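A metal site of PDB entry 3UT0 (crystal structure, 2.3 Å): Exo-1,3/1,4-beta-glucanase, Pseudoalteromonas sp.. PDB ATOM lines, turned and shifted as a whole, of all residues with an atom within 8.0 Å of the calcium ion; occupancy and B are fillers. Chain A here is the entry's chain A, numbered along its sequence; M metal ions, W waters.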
ATOM      1  N   VAL A 166      16.094 -36.604  18.067  1.00  0.00           N
ATOM      2  CA  VAL A 166      15.948 -36.445  19.518  1.00  0.00           C
ATOM      3  C   VAL A 166      15.088 -35.247  19.909  1.00  0.00           C
ATOM      4  O   VAL A 166      15.385 -34.109  19.564  1.00  0.00           O
ATOM      5  CB  VAL A 166      17.332 -36.382  20.204  1.00  0.00           C
ATOM      6  CG1 VAL A 166      17.207 -36.046  21.685  1.00  0.00           C
ATOM      7  CG2 VAL A 166      18.067 -37.700  20.010  1.00  0.00           C
ATOM      8  N   ARG A 167      14.061 -35.521  20.705  1.00  0.00           N
ATOM      9  CA  ARG A 167      13.036 -34.526  21.032  1.00  0.00           C
ATOM     10  C   ARG A 167      13.112 -34.026  22.462  1.00  0.00           C
ATOM     11  O   ARG A 167      12.502 -33.002  22.804  1.00  0.00           O
ATOM     12  CB  ARG A 167      11.638 -35.106  20.757  1.00  0.00           C
ATOM     13  CG  ARG A 167      11.484 -35.747  19.371  1.00  0.00           C
ATOM     14  CD  ARG A 167      11.557 -34.686  18.285  1.00  0.00           C
ATOM     15  NE  ARG A 167      10.330 -33.914  18.199  1.00  0.00           N
ATOM     16  CZ  ARG A 167      10.111 -32.969  17.300  1.00  0.00           C
ATOM     17  NH1 ARG A 167      11.070 -32.629  16.441  1.00  0.00           N
ATOM     18  NH2 ARG A 167       8.961 -32.317  17.277  1.00  0.00           N
ATOM     19  N   ASP A 168      13.897 -34.703  23.288  1.00  0.00           N
ATOM     20  CA  ASP A 168      14.074 -34.311  24.690  1.00  0.00           C
ATOM     21  C   ASP A 168      15.530 -34.505  25.053  1.00  0.00           C
ATOM     22  O   ASP A 168      16.024 -35.636  25.105  1.00  0.00           O
ATOM     23  CB  ASP A 168      13.168 -35.156  25.589  1.00  0.00           C
ATOM     24  CG  ASP A 168      13.126 -34.643  27.043  1.00  0.00           C
ATOM     25  OD1 ASP A 168      14.183 -34.218  27.571  1.00  0.00           O
ATOM     26  OD2 ASP A 168      12.024 -34.631  27.640  1.00  0.00           O
ATOM     27  N   ASP A 169      16.230 -33.397  25.273  1.00  0.00           N
ATOM     28  CA  ASP A 169      17.679 -33.410  25.421  1.00  0.00           C
ATOM     29  C   ASP A 169      18.193 -34.027  26.713  1.00  0.00           C
ATOM     30  O   ASP A 169      19.393 -34.208  26.891  1.00  0.00           O
ATOM     31  CB  ASP A 169      18.246 -32.002  25.289  1.00  0.00           C
ATOM     32  CG  ASP A 169      17.979 -31.387  23.924  1.00  0.00           C
ATOM     33  OD1 ASP A 169      17.657 -32.131  22.971  1.00  0.00           O
ATOM     34  OD2 ASP A 169      18.055 -30.140  23.817  1.00  0.00           O
ATOM     35  N   THR A 174      21.648 -38.079  23.276  1.00  0.00           N
ATOM     36  CA  THR A 174      21.322 -36.949  22.412  1.00  0.00           C
ATOM     37  C   THR A 174      22.413 -36.609  21.379  1.00  0.00           C
ATOM     38  O   THR A 174      22.102 -36.241  20.252  1.00  0.00           O
ATOM     39  CB  THR A 174      21.007 -35.697  23.260  1.00  0.00           C
ATOM     40  OG1 THR A 174      19.823 -35.936  24.044  1.00  0.00           O
ATOM     41  CG2 THR A 174      20.781 -34.479  22.387  1.00  0.00           C
ATOM     42  N   SER A 179      20.107 -34.141  14.705  1.00  0.00           N
ATOM     43  CA  SER A 179      19.120 -33.068  14.796  1.00  0.00           C
ATOM     44  C   SER A 179      17.876 -33.447  15.597  1.00  0.00           C
ATOM     45  O   SER A 179      17.586 -34.624  15.764  1.00  0.00           O
ATOM     46  CB  SER A 179      18.683 -32.655  13.376  1.00  0.00           C
ATOM     47  OG  SER A 179      17.759 -31.582  13.411  1.00  0.00           O
ATOM     48  N   GLU A 180      17.197 -32.440  16.168  1.00  0.00           N
ATOM     49  CA  GLU A 180      15.875 -32.670  16.738  1.00  0.00           C
ATOM     50  C   GLU A 180      14.781 -32.788  15.666  1.00  0.00           C
ATOM     51  O   GLU A 180      13.667 -33.226  15.921  1.00  0.00           O
ATOM     52  CB  GLU A 180      15.521 -31.505  17.668  1.00  0.00           C
ATOM     53  CG  GLU A 180      15.288 -30.176  16.971  1.00  0.00           C
ATOM     54  CD  GLU A 180      15.162 -28.992  17.922  1.00  0.00           C
ATOM     55  OE1 GLU A 180      15.762 -29.039  19.007  1.00  0.00           O
ATOM     56  OE2 GLU A 180      14.448 -28.018  17.590  1.00  0.00           O
ATOM     57  N   ASP A 181      15.117 -32.299  14.477  1.00  0.00           N
ATOM     58  CA  ASP A 181      14.263 -32.145  13.304  1.00  0.00           C
ATOM     59  C   ASP A 181      14.487 -33.337  12.339  1.00  0.00           C
ATOM     60  O   ASP A 181      15.643 -33.579  12.010  1.00  0.00           O
ATOM     61  CB  ASP A 181      14.594 -30.872  12.571  1.00  0.00           C
ATOM     62  CG  ASP A 181      13.754 -30.697  11.337  1.00  0.00           C
ATOM     63  OD1 ASP A 181      12.657 -31.275  11.264  1.00  0.00           O
ATOM     64  OD2 ASP A 181      14.263 -30.135  10.357  1.00  0.00           O
ATOM     65  N   PRO A 534      22.368 -29.046  23.880  1.00  0.00           N
ATOM     66  CA  PRO A 534      22.194 -27.758  24.535  1.00  0.00           C
ATOM     67  C   PRO A 534      21.897 -27.972  26.020  1.00  0.00           C
ATOM     68  O   PRO A 534      21.310 -28.994  26.363  1.00  0.00           O
ATOM     69  CB  PRO A 534      20.953 -27.186  23.845  1.00  0.00           C
ATOM     70  CG  PRO A 534      20.848 -27.923  22.557  1.00  0.00           C
ATOM     71  CD  PRO A 534      21.335 -29.297  22.862  1.00  0.00           C
ATOM     72  N   SER A 581      21.337 -27.337  15.170  1.00  0.00           N
ATOM     73  CA  SER A 581      20.441 -28.404  14.760  1.00  0.00           C
ATOM     74  C   SER A 581      19.579 -28.839  15.949  1.00  0.00           C
ATOM     75  O   SER A 581      18.708 -29.688  15.819  1.00  0.00           O
ATOM     76  CB  SER A 581      21.208 -29.582  14.162  1.00  0.00           C
ATOM     77  OG  SER A 581      21.996 -30.192  15.162  1.00  0.00           O
ATOM     78  N   PHE A 582      19.826 -28.217  17.099  1.00  0.00           N
ATOM     79  CA  PHE A 582      19.019 -28.369  18.292  1.00  0.00           C
ATOM     80  C   PHE A 582      18.683 -27.003  18.875  1.00  0.00           C
ATOM     81  O   PHE A 582      19.548 -26.128  18.952  1.00  0.00           O
ATOM     82  CB  PHE A 582      19.790 -29.160  19.346  1.00  0.00           C
ATOM     83  CG  PHE A 582      19.849 -30.638  19.089  1.00  0.00           C
ATOM     84  CD1 PHE A 582      19.020 -31.499  19.792  1.00  0.00           C
ATOM     85  CD2 PHE A 582      20.668 -31.149  18.093  1.00  0.00           C
ATOM     86  CE1 PHE A 582      19.069 -32.875  19.557  1.00  0.00           C
ATOM     87  CE2 PHE A 582      20.709 -32.517  17.849  1.00  0.00           C
ATOM     88  CZ  PHE A 582      19.912 -33.382  18.577  1.00  0.00           C
ATOM     89  N   SER A 583      17.444 -26.815  19.318  1.00  0.00           N
ATOM     90  CA  SER A 583      17.051 -25.531  19.900  1.00  0.00           C
ATOM     91  C   SER A 583      17.718 -25.354  21.255  1.00  0.00           C
ATOM     92  O   SER A 583      17.859 -26.299  22.017  1.00  0.00           O
ATOM     93  CB  SER A 583      15.538 -25.447  20.056  1.00  0.00           C
ATOM     94  OG  SER A 583      14.877 -25.579  18.807  1.00  0.00           O
ATOM     95  N   TRP A 584      18.137 -24.127  21.546  1.00  0.00           N
ATOM     96  CA  TRP A 584      18.828 -23.837  22.799  1.00  0.00           C
ATOM     97  C   TRP A 584      17.831 -23.243  23.801  1.00  0.00           C
ATOM     98  O   TRP A 584      17.110 -22.294  23.486  1.00  0.00           O
ATOM     99  CB  TRP A 584      20.000 -22.886  22.572  1.00  0.00           C
ATOM    100  CG  TRP A 584      21.029 -23.017  23.647  1.00  0.00           C
ATOM    101  CD1 TRP A 584      20.981 -22.512  24.916  1.00  0.00           C
ATOM    102  CD2 TRP A 584      22.254 -23.745  23.545  1.00  0.00           C
ATOM    103  NE1 TRP A 584      22.111 -22.871  25.601  1.00  0.00           N
ATOM    104  CE2 TRP A 584      22.913 -23.627  24.785  1.00  0.00           C
ATOM    105  CE3 TRP A 584      22.877 -24.460  22.514  1.00  0.00           C
ATOM    106  CZ2 TRP A 584      24.158 -24.212  25.026  1.00  0.00           C
ATOM    107  CZ3 TRP A 584      24.103 -25.040  22.764  1.00  0.00           C
ATOM    108  CH2 TRP A 584      24.734 -24.910  24.004  1.00  0.00           C
ATOM    109  N   PRO A 585      17.755 -23.821  25.010  1.00  0.00           N
ATOM    110  CA  PRO A 585      16.727 -23.444  25.988  1.00  0.00           C
ATOM    111  C   PRO A 585      16.976 -22.086  26.651  1.00  0.00           C
ATOM    112  O   PRO A 585      18.117 -21.734  26.970  1.00  0.00           O
ATOM    113  CB  PRO A 585      16.813 -24.561  27.019  1.00  0.00           C
ATOM    114  CG  PRO A 585      18.217 -24.994  26.972  1.00  0.00           C
ATOM    115  CD  PRO A 585      18.597 -24.924  25.511  1.00  0.00           C
ATOM    116  N   GLN A 590      12.666 -26.077  29.912  1.00  0.00           N
ATOM    117  CA  GLN A 590      12.220 -26.248  28.539  1.00  0.00           C
ATOM    118  C   GLN A 590      12.708 -27.577  27.993  1.00  0.00           C
ATOM    119  O   GLN A 590      13.590 -27.623  27.136  1.00  0.00           O
ATOM    120  CB  GLN A 590      12.724 -25.085  27.690  1.00  0.00           C
ATOM    121  CG  GLN A 590      11.840 -23.848  27.748  1.00  0.00           C
ATOM    122  CD  GLN A 590      12.356 -22.739  26.862  1.00  0.00           C
ATOM    123  OE1 GLN A 590      13.554 -22.483  26.802  1.00  0.00           O
ATOM    124  NE2 GLN A 590      11.443 -22.081  26.155  1.00  0.00           N
ATOM    125  N   PHE A 591      12.109 -28.652  28.490  1.00  0.00           N
ATOM    126  CA  PHE A 591      12.598 -30.005  28.253  1.00  0.00           C
ATOM    127  C   PHE A 591      12.289 -30.482  26.834  1.00  0.00           C
ATOM    128  O   PHE A 591      13.064 -31.249  26.237  1.00  0.00           O
ATOM    129  CB  PHE A 591      12.041 -30.994  29.273  1.00  0.00           C
ATOM    130  CG  PHE A 591      12.448 -30.701  30.689  1.00  0.00           C
ATOM    131  CD1 PHE A 591      13.782 -30.759  31.068  1.00  0.00           C
ATOM    132  CD2 PHE A 591      11.504 -30.415  31.660  1.00  0.00           C
ATOM    133  CE1 PHE A 591      14.168 -30.505  32.365  1.00  0.00           C
ATOM    134  CE2 PHE A 591      11.878 -30.156  32.972  1.00  0.00           C
ATOM    135  CZ  PHE A 591      13.217 -30.201  33.323  1.00  0.00           C
ATOM    136  N   THR A 592      11.181 -30.006  26.281  1.00  0.00           N
ATOM    137  CA  THR A 592      10.823 -30.454  24.944  1.00  0.00           C
ATOM    138  C   THR A 592      10.628 -29.276  24.018  1.00  0.00           C
ATOM    139  O   THR A 592       9.507 -28.931  23.644  1.00  0.00           O
ATOM    140  CB  THR A 592       9.520 -31.311  24.960  1.00  0.00           C
ATOM    141  OG1 THR A 592       8.498 -30.617  25.685  1.00  0.00           O
ATOM    142  CG2 THR A 592       9.754 -32.660  25.626  1.00  0.00           C
ATOM    143  N   LEU A 593      11.742 -28.589  23.750  1.00  0.00           N
ATOM    144  CA  LEU A 593      11.753 -27.406  22.899  1.00  0.00           C
ATOM    145  C   LEU A 593      12.210 -27.802  21.470  1.00  0.00           C
ATOM    146  O   LEU A 593      13.409 -28.030  21.220  1.00  0.00           O
ATOM    147  CB  LEU A 593      12.757 -26.433  23.516  1.00  0.00           C
ATOM    148  CG  LEU A 593      13.059 -25.107  22.847  1.00  0.00           C
ATOM    149  CD1 LEU A 593      11.841 -24.221  22.948  1.00  0.00           C
ATOM    150  CD2 LEU A 593      14.248 -24.472  23.517  1.00  0.00           C
ATOM    151  N   ASN A 594      11.277 -27.864  20.525  1.00  0.00           N
ATOM    152  CA  ASN A 594      11.638 -28.328  19.164  1.00  0.00           C
ATOM    153  C   ASN A 594      11.062 -27.434  18.065  1.00  0.00           C
ATOM    154  O   ASN A 594       9.967 -26.897  18.243  1.00  0.00           O
ATOM    155  CB  ASN A 594      11.178 -29.764  18.971  1.00  0.00           C
ATOM    156  CG  ASN A 594      11.883 -30.715  19.914  1.00  0.00           C
ATOM    157  OD1 ASN A 594      13.107 -30.799  19.944  1.00  0.00           O
ATOM    158  ND2 ASN A 594      11.104 -31.429  20.719  1.00  0.00           N
ATOM    159  N   LEU A 595      11.767 -27.264  16.945  1.00  0.00           N
ATOM    160  CA  LEU A 595      11.228 -26.374  15.901  1.00  0.00           C
ATOM    161  C   LEU A 595       9.872 -26.881  15.437  1.00  0.00           C
ATOM    162  O   LEU A 595       9.599 -28.099  15.449  1.00  0.00           O
ATOM    163  CB  LEU A 595      12.151 -26.254  14.690  1.00  0.00           C
ATOM    164  CG  LEU A 595      12.019 -27.158  13.468  1.00  0.00           C
ATOM    165  CD1 LEU A 595      12.866 -26.588  12.336  1.00  0.00           C
ATOM    166  CD2 LEU A 595      12.305 -28.601  13.763  1.00  0.00           C
ATOM    167  N   ASP A 597       7.215 -26.418  17.044  1.00  0.00           N
ATOM    168  CA  ASP A 597       6.362 -26.525  18.238  1.00  0.00           C
ATOM    169  C   ASP A 597       5.397 -25.347  18.269  1.00  0.00           C
ATOM    170  O   ASP A 597       5.734 -24.255  17.789  1.00  0.00           O
ATOM    171  CB  ASP A 597       7.196 -26.545  19.529  1.00  0.00           C
ATOM    172  CG  ASP A 597       7.689 -27.926  19.880  1.00  0.00           C
ATOM    173  OD1 ASP A 597       7.387 -28.891  19.153  1.00  0.00           O
ATOM    174  OD2 ASP A 597       8.472 -28.051  20.845  1.00  0.00           O
ATOM    175  N   TYR A 600       6.922 -21.936  20.877  1.00  0.00           N
ATOM    176  CA  TYR A 600       8.348 -22.074  20.610  1.00  0.00           C
ATOM    177  C   TYR A 600       9.061 -20.813  21.072  1.00  0.00           C
ATOM    178  O   TYR A 600       9.013 -19.779  20.400  1.00  0.00           O
ATOM    179  CB  TYR A 600       8.601 -22.334  19.120  1.00  0.00           C
ATOM    180  CG  TYR A 600      10.029 -22.666  18.743  1.00  0.00           C
ATOM    181  CD1 TYR A 600      10.727 -21.903  17.793  1.00  0.00           C
ATOM    182  CD2 TYR A 600      10.686 -23.765  19.298  1.00  0.00           C
ATOM    183  CE1 TYR A 600      12.033 -22.210  17.444  1.00  0.00           C
ATOM    184  CE2 TYR A 600      11.991 -24.082  18.952  1.00  0.00           C
ATOM    185  CZ  TYR A 600      12.658 -23.299  18.024  1.00  0.00           C
ATOM    186  OH  TYR A 600      13.963 -23.606  17.675  1.00  0.00           O
ATOM    187  N   TYR A 606      16.505 -23.133  16.464  1.00  0.00           N
ATOM    188  CA  TYR A 606      17.027 -24.004  15.426  1.00  0.00           C
ATOM    189  C   TYR A 606      17.485 -23.138  14.244  1.00  0.00           C
ATOM    190  O   TYR A 606      16.739 -22.251  13.803  1.00  0.00           O
ATOM    191  CB  TYR A 606      15.910 -24.947  14.947  1.00  0.00           C
ATOM    192  CG  TYR A 606      16.322 -25.889  13.838  1.00  0.00           C
ATOM    193  CD1 TYR A 606      16.783 -27.164  14.153  1.00  0.00           C
ATOM    194  CD2 TYR A 606      16.258 -25.528  12.497  1.00  0.00           C
ATOM    195  CE1 TYR A 606      17.161 -28.063  13.171  1.00  0.00           C
ATOM    196  CE2 TYR A 606      16.647 -26.423  11.497  1.00  0.00           C
ATOM    197  CZ  TYR A 606      17.100 -27.688  11.841  1.00  0.00           C
ATOM    198  OH  TYR A 606      17.488 -28.572  10.875  1.00  0.00           O
HETATM  199 CA    CA M   1      14.869 -29.820  21.028  1.00  0.00          CA
HETATM  200  O   HOH W   1      16.783 -28.873  22.096  1.00  0.00           O
HETATM  201  O   HOH W   2      15.789 -32.008  21.316  1.00  0.00           O
HETATM  202  O   HOH W   3      14.004 -30.430  23.283  1.00  0.00           O
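Of the 23 residues printed, 3 come within 4 Å of the calcium ion.
Along chain A the residues within 4 Å of the calcium ion span positions 180 to 594.
Water W1 bridges the side-chain carboxylate of Asp 169 (2.5 Å) and the backbone carbonyl oxygen of Ser 583 (2.8 Å).
Water W2 lies within hydrogen-bond range of the side-chain carboxylate of Asp 169 and the backbone carbonyl oxygen of Val 166.
Water W3 lies within hydrogen-bond range of the backbone NH of Leu 593 (3.0 Å), the backbone carbonyl oxygen of Arg 167 (3.0 Å) and the backbone carbonyl oxygen of Phe 591 (3.2 Å).
The calcium ion is bound by the side-chain amide oxygen (OD1) of Asn 594 (2.3 Å), the backbone carbonyl oxygen (O) of Leu 593 (2.3 Å), the side-chain carboxylate (OE1) of Glu 180 (2.3 Å), water W1 (2.4 Å), water W2 (2.4 Å) and water W3 (2.5 Å).
ND2 of Asn 594 sits at hydrogen-bond distance from O of Arg 167, at 3.0 Å.
The side-chain carboxylate (OD2) of Asp 597 sits at hydrogen-bond distance from the backbone NH (N) of Asn 594 (2.8 Å).
OG of Ser 583 lies within hydrogen-bond range of OE2 of Glu 180, at 2.8 Å.
The guanidinium group (NH1) of Arg 167 sits at hydrogen-bond distance from the backbone carbonyl oxygen (O) of Glu 180, at 2.7 Å.
The side-chain carboxylate (OE2) of Glu 180 lies within hydrogen-bond range of the backbone NH (N) of Leu 595.
N of Glu 180 lies within hydrogen-bond range of O of Ser 581 (3.2 Å).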
